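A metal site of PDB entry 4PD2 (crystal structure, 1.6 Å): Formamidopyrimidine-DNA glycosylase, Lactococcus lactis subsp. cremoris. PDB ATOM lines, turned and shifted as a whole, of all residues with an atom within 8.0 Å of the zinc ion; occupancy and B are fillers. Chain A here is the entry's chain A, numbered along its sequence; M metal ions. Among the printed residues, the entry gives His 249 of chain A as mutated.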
ATOM      1  N   TRP A 179      17.130 -27.565 -12.256  1.00  0.00           N
ATOM      2  CA  TRP A 179      18.431 -28.274 -12.267  1.00  0.00           C
ATOM      3  C   TRP A 179      18.366 -29.582 -11.444  1.00  0.00           C
ATOM      4  O   TRP A 179      18.824 -30.634 -11.854  1.00  0.00           O
ATOM      5  CB  TRP A 179      19.516 -27.343 -11.711  1.00  0.00           C
ATOM      6  CG  TRP A 179      20.892 -28.049 -11.619  1.00  0.00           C
ATOM      7  CD1 TRP A 179      21.828 -28.122 -12.604  1.00  0.00           C
ATOM      8  CD2 TRP A 179      21.406 -28.742 -10.492  1.00  0.00           C
ATOM      9  NE1 TRP A 179      22.933 -28.845 -12.141  1.00  0.00           N
ATOM     10  CE2 TRP A 179      22.698 -29.223 -10.848  1.00  0.00           C
ATOM     11  CE3 TRP A 179      20.893 -29.023  -9.223  1.00  0.00           C
ATOM     12  CZ2 TRP A 179      23.503 -29.963  -9.962  1.00  0.00           C
ATOM     13  CZ3 TRP A 179      21.685 -29.764  -8.347  1.00  0.00           C
ATOM     14  CH2 TRP A 179      22.982 -30.236  -8.712  1.00  0.00           C
ATOM     15  N   LYS A 182      16.493 -32.124 -13.266  1.00  0.00           N
ATOM     16  CA  LYS A 182      17.087 -32.458 -14.563  1.00  0.00           C
ATOM     17  C   LYS A 182      16.145 -32.161 -15.742  1.00  0.00           C
ATOM     18  O   LYS A 182      16.035 -32.956 -16.697  1.00  0.00           O
ATOM     19  CB  LYS A 182      17.513 -33.917 -14.568  1.00  0.00           C
ATOM     20  CG  LYS A 182      18.649 -34.143 -13.569  1.00  0.00           C
ATOM     21  CD  LYS A 182      18.886 -35.671 -13.353  1.00  0.00           C
ATOM     22  CE  LYS A 182      19.867 -35.899 -12.233  1.00  0.00           C
ATOM     23  NZ  LYS A 182      19.899 -37.334 -11.819  1.00  0.00           N
ATOM     24  N   VAL A 237      22.985 -23.476  -9.170  1.00  0.00           N
ATOM     25  CA  VAL A 237      23.017 -22.920 -10.533  1.00  0.00           C
ATOM     26  C   VAL A 237      22.727 -21.444 -10.596  1.00  0.00           C
ATOM     27  O   VAL A 237      23.322 -20.737 -11.412  1.00  0.00           O
ATOM     28  CB  VAL A 237      22.017 -23.644 -11.550  1.00  0.00           C
ATOM     29  CG1 VAL A 237      22.489 -25.050 -11.881  1.00  0.00           C
ATOM     30  CG2 VAL A 237      20.527 -23.626 -11.064  1.00  0.00           C
ATOM     31  N   LYS A 244      31.513 -24.733 -12.770  1.00  0.00           N
ATOM     32  CA  LYS A 244      31.211 -26.112 -13.160  1.00  0.00           C
ATOM     33  C   LYS A 244      29.966 -26.631 -12.474  1.00  0.00           C
ATOM     34  O   LYS A 244      29.701 -26.291 -11.307  1.00  0.00           O
ATOM     35  CB  LYS A 244      32.385 -27.017 -12.830  1.00  0.00           C
ATOM     36  CG  LYS A 244      33.609 -26.678 -13.598  1.00  0.00           C
ATOM     37  CD  LYS A 244      33.462 -27.029 -15.033  1.00  0.00           C
ATOM     38  CE  LYS A 244      34.844 -27.162 -15.692  1.00  0.00           C
ATOM     39  NZ  LYS A 244      34.769 -27.117 -17.218  1.00  0.00           N
ATOM     40  N   CYS A 245      29.187 -27.436 -13.200  1.00  0.00           N
ATOM     41  CA  CYS A 245      28.046 -28.148 -12.589  1.00  0.00           C
ATOM     42  C   CYS A 245      28.553 -29.001 -11.429  1.00  0.00           C
ATOM     43  O   CYS A 245      29.585 -29.649 -11.511  1.00  0.00           O
ATOM     44  CB  CYS A 245      27.319 -29.020 -13.621  1.00  0.00           C
ATOM     45  SG  CYS A 245      25.995 -30.041 -12.913  1.00  0.00           S
ATOM     46  N   SER A 246      27.819 -28.955 -10.316  1.00  0.00           N
ATOM     47  CA  SER A 246      28.316 -29.646  -9.138  1.00  0.00           C
ATOM     48  C   SER A 246      28.196 -31.164  -9.247  1.00  0.00           C
ATOM     49  O   SER A 246      28.752 -31.867  -8.426  1.00  0.00           O
ATOM     50  CB  SER A 246      27.583 -29.170  -7.887  1.00  0.00           C
ATOM     51  OG  SER A 246      26.226 -29.568  -7.922  1.00  0.00           O
ATOM     52  N   ARG A 247      27.480 -31.683 -10.236  1.00  0.00           N
ATOM     53  CA  ARG A 247      27.458 -33.130 -10.433  1.00  0.00           C
ATOM     54  C   ARG A 247      28.742 -33.661 -11.093  1.00  0.00           C
ATOM     55  O   ARG A 247      28.885 -34.848 -11.254  1.00  0.00           O
ATOM     56  CB  ARG A 247      26.233 -33.539 -11.242  1.00  0.00           C
ATOM     57  CG  ARG A 247      24.962 -33.423 -10.372  1.00  0.00           C
ATOM     58  CD  ARG A 247      23.729 -33.405 -11.206  1.00  0.00           C
ATOM     59  NE  ARG A 247      22.526 -33.558 -10.394  1.00  0.00           N
ATOM     60  CZ  ARG A 247      21.380 -32.964 -10.667  1.00  0.00           C
ATOM     61  NH1 ARG A 247      20.306 -33.156  -9.862  1.00  0.00           N
ATOM     62  NH2 ARG A 247      21.286 -32.178 -11.736  1.00  0.00           N
ATOM     63  N   GLY A 248      29.607 -32.750 -11.486  1.00  0.00           N
ATOM     64  CA  GLY A 248      31.020 -33.017 -11.722  1.00  0.00           C
ATOM     65  C   GLY A 248      31.355 -33.658 -13.055  1.00  0.00           C
ATOM     66  O   GLY A 248      32.331 -34.390 -13.132  1.00  0.00           O
ATOM     67  N   HIS A 249      30.566 -33.394 -14.087  1.00  0.00           N
ATOM     68  CA  HIS A 249      30.889 -33.851 -15.437  1.00  0.00           C
ATOM     69  C   HIS A 249      31.588 -32.736 -16.252  1.00  0.00           C
ATOM     70  O   HIS A 249      31.640 -32.773 -17.467  1.00  0.00           O
ATOM     71  CB  HIS A 249      29.655 -34.376 -16.185  1.00  0.00           C
ATOM     72  CG  HIS A 249      28.322 -33.763 -15.786  1.00  0.00           C
ATOM     73  ND1 HIS A 249      27.253 -34.540 -15.430  1.00  0.00           N
ATOM     74  CD2 HIS A 249      27.892 -32.479 -15.750  1.00  0.00           C
ATOM     75  CE1 HIS A 249      26.205 -33.770 -15.154  1.00  0.00           C
ATOM     76  NE2 HIS A 249      26.570 -32.507 -15.313  1.00  0.00           N
ATOM     77  N   GLY A 250      32.127 -31.762 -15.548  1.00  0.00           N
ATOM     78  CA  GLY A 250      32.849 -30.695 -16.188  1.00  0.00           C
ATOM     79  C   GLY A 250      32.066 -29.725 -17.073  1.00  0.00           C
ATOM     80  O   GLY A 250      32.676 -28.867 -17.690  1.00  0.00           O
ATOM     81  N   ALA A 251      30.739 -29.817 -17.145  1.00  0.00           N
ATOM     82  CA  ALA A 251      29.991 -28.829 -17.926  1.00  0.00           C
ATOM     83  C   ALA A 251      29.937 -27.513 -17.122  1.00  0.00           C
ATOM     84  O   ALA A 251      29.757 -27.555 -15.931  1.00  0.00           O
ATOM     85  CB  ALA A 251      28.579 -29.296 -18.247  1.00  0.00           C
ATOM     86  N   GLU A 252      30.050 -26.375 -17.802  1.00  0.00           N
ATOM     87  CA  GLU A 252      29.801 -25.073 -17.133  1.00  0.00           C
ATOM     88  C   GLU A 252      28.345 -24.765 -17.093  1.00  0.00           C
ATOM     89  O   GLU A 252      27.598 -25.047 -18.050  1.00  0.00           O
ATOM     90  CB  GLU A 252      30.486 -23.902 -17.867  1.00  0.00           C
ATOM     91  CG  GLU A 252      32.022 -24.020 -17.903  1.00  0.00           C
ATOM     92  CD  GLU A 252      32.712 -22.739 -18.383  1.00  0.00           C
ATOM     93  OE1 GLU A 252      32.019 -21.821 -18.922  1.00  0.00           O
ATOM     94  OE2 GLU A 252      33.953 -22.626 -18.237  1.00  0.00           O
ATOM     95  N   ILE A 253      27.921 -24.139 -16.018  1.00  0.00           N
ATOM     96  CA  ILE A 253      26.572 -23.557 -15.999  1.00  0.00           C
ATOM     97  C   ILE A 253      26.464 -22.435 -17.039  1.00  0.00           C
ATOM     98  O   ILE A 253      27.347 -21.560 -17.164  1.00  0.00           O
ATOM     99  CB  ILE A 253      26.271 -23.035 -14.617  1.00  0.00           C
ATOM    100  CG1 ILE A 253      26.379 -24.221 -13.630  1.00  0.00           C
ATOM    101  CG2 ILE A 253      24.887 -22.352 -14.550  1.00  0.00           C
ATOM    102  CD1 ILE A 253      25.521 -25.475 -14.019  1.00  0.00           C
ATOM    103  N   PHE A 265      21.377 -22.864 -16.136  1.00  0.00           N
ATOM    104  CA  PHE A 265      21.122 -24.315 -16.234  1.00  0.00           C
ATOM    105  C   PHE A 265      22.403 -25.044 -16.614  1.00  0.00           C
ATOM    106  O   PHE A 265      23.355 -24.415 -17.128  1.00  0.00           O
ATOM    107  CB  PHE A 265      20.014 -24.622 -17.247  1.00  0.00           C
ATOM    108  CG  PHE A 265      20.440 -24.422 -18.683  1.00  0.00           C
ATOM    109  CD1 PHE A 265      20.629 -23.110 -19.189  1.00  0.00           C
ATOM    110  CD2 PHE A 265      20.649 -25.521 -19.508  1.00  0.00           C
ATOM    111  CE1 PHE A 265      21.063 -22.930 -20.548  1.00  0.00           C
ATOM    112  CE2 PHE A 265      21.066 -25.373 -20.832  1.00  0.00           C
ATOM    113  CZ  PHE A 265      21.272 -24.070 -21.350  1.00  0.00           C
ATOM    114  N   CYS A 266      22.431 -26.347 -16.369  1.00  0.00           N
ATOM    115  CA  CYS A 266      23.529 -27.191 -16.831  1.00  0.00           C
ATOM    116  C   CYS A 266      23.065 -27.878 -18.124  1.00  0.00           C
ATOM    117  O   CYS A 266      22.089 -28.620 -18.107  1.00  0.00           O
ATOM    118  CB  CYS A 266      23.865 -28.265 -15.773  1.00  0.00           C
ATOM    119  SG  CYS A 266      25.066 -29.450 -16.509  1.00  0.00           S
ATOM    120  N   PRO A 267      23.757 -27.622 -19.254  1.00  0.00           N
ATOM    121  CA  PRO A 267      23.275 -28.217 -20.510  1.00  0.00           C
ATOM    122  C   PRO A 267      23.477 -29.727 -20.596  1.00  0.00           C
ATOM    123  O   PRO A 267      22.902 -30.326 -21.477  1.00  0.00           O
ATOM    124  CB  PRO A 267      24.134 -27.558 -21.588  1.00  0.00           C
ATOM    125  CG  PRO A 267      24.854 -26.468 -20.924  1.00  0.00           C
ATOM    126  CD  PRO A 267      24.949 -26.800 -19.449  1.00  0.00           C
ATOM    127  N   VAL A 268      24.247 -30.321 -19.704  1.00  0.00           N
ATOM    128  CA  VAL A 268      24.334 -31.821 -19.687  1.00  0.00           C
ATOM    129  C   VAL A 268      23.161 -32.396 -18.890  1.00  0.00           C
ATOM    130  O   VAL A 268      22.467 -33.281 -19.365  1.00  0.00           O
ATOM    131  CB  VAL A 268      25.655 -32.297 -19.098  1.00  0.00           C
ATOM    132  CG1 VAL A 268      25.668 -33.843 -18.947  1.00  0.00           C
ATOM    133  CG2 VAL A 268      26.770 -31.873 -20.055  1.00  0.00           C
ATOM    134  N   CYS A 269      22.924 -31.875 -17.680  1.00  0.00           N
ATOM    135  CA  CYS A 269      21.821 -32.337 -16.832  1.00  0.00           C
ATOM    136  C   CYS A 269      20.454 -32.041 -17.403  1.00  0.00           C
ATOM    137  O   CYS A 269      19.515 -32.802 -17.156  1.00  0.00           O
ATOM    138  CB  CYS A 269      21.863 -31.644 -15.458  1.00  0.00           C
ATOM    139  SG  CYS A 269      23.254 -32.165 -14.419  1.00  0.00           S
ATOM    140  N   GLN A 270      20.334 -30.953 -18.143  1.00  0.00           N
ATOM    141  CA  GLN A 270      19.007 -30.417 -18.499  1.00  0.00           C
ATOM    142  C   GLN A 270      18.936 -30.353 -20.001  1.00  0.00           C
ATOM    143  O   GLN A 270      19.319 -29.365 -20.616  1.00  0.00           O
ATOM    144  CB  GLN A 270      18.815 -29.019 -17.894  1.00  0.00           C
ATOM    145  CG  GLN A 270      18.742 -29.081 -16.392  1.00  0.00           C
ATOM    146  CD  GLN A 270      18.885 -27.721 -15.702  1.00  0.00           C
ATOM    147  OE1 GLN A 270      19.972 -27.343 -15.275  1.00  0.00           O
ATOM    148  NE2 GLN A 270      17.770 -26.993 -15.545  1.00  0.00           N
HETATM  149 ZN    ZN M   1      25.223 -31.023 -14.859  1.00  0.00          ZN
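The zinc ion is bound by NE2 of His 249, SG of Cys 266, SG of Cys 245 and SG of Cys 269.
SG of Cys 266 sits close to N of Val 268 (3.4 Å).
N of Cys 266 lies within hydrogen-bond range of OE1 of Gln 270 (2.9 Å).
The side-chain sulfur (SG) of Cys 245 lies close to the indole nitrogen (NE1) of Trp 179, 3.4 Å away.
SG of Cys 245 lies close to N of Arg 247 (3.5 Å).
The backbone NH (N) of Cys 245 lies within hydrogen-bond range of the backbone carbonyl oxygen (O) of Ala 251 (2.8 Å).
The side-chain sulfur (SG) of Cys 269 lies close to the guanidinium group (NH2) of Arg 247, 3.3 Å away.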
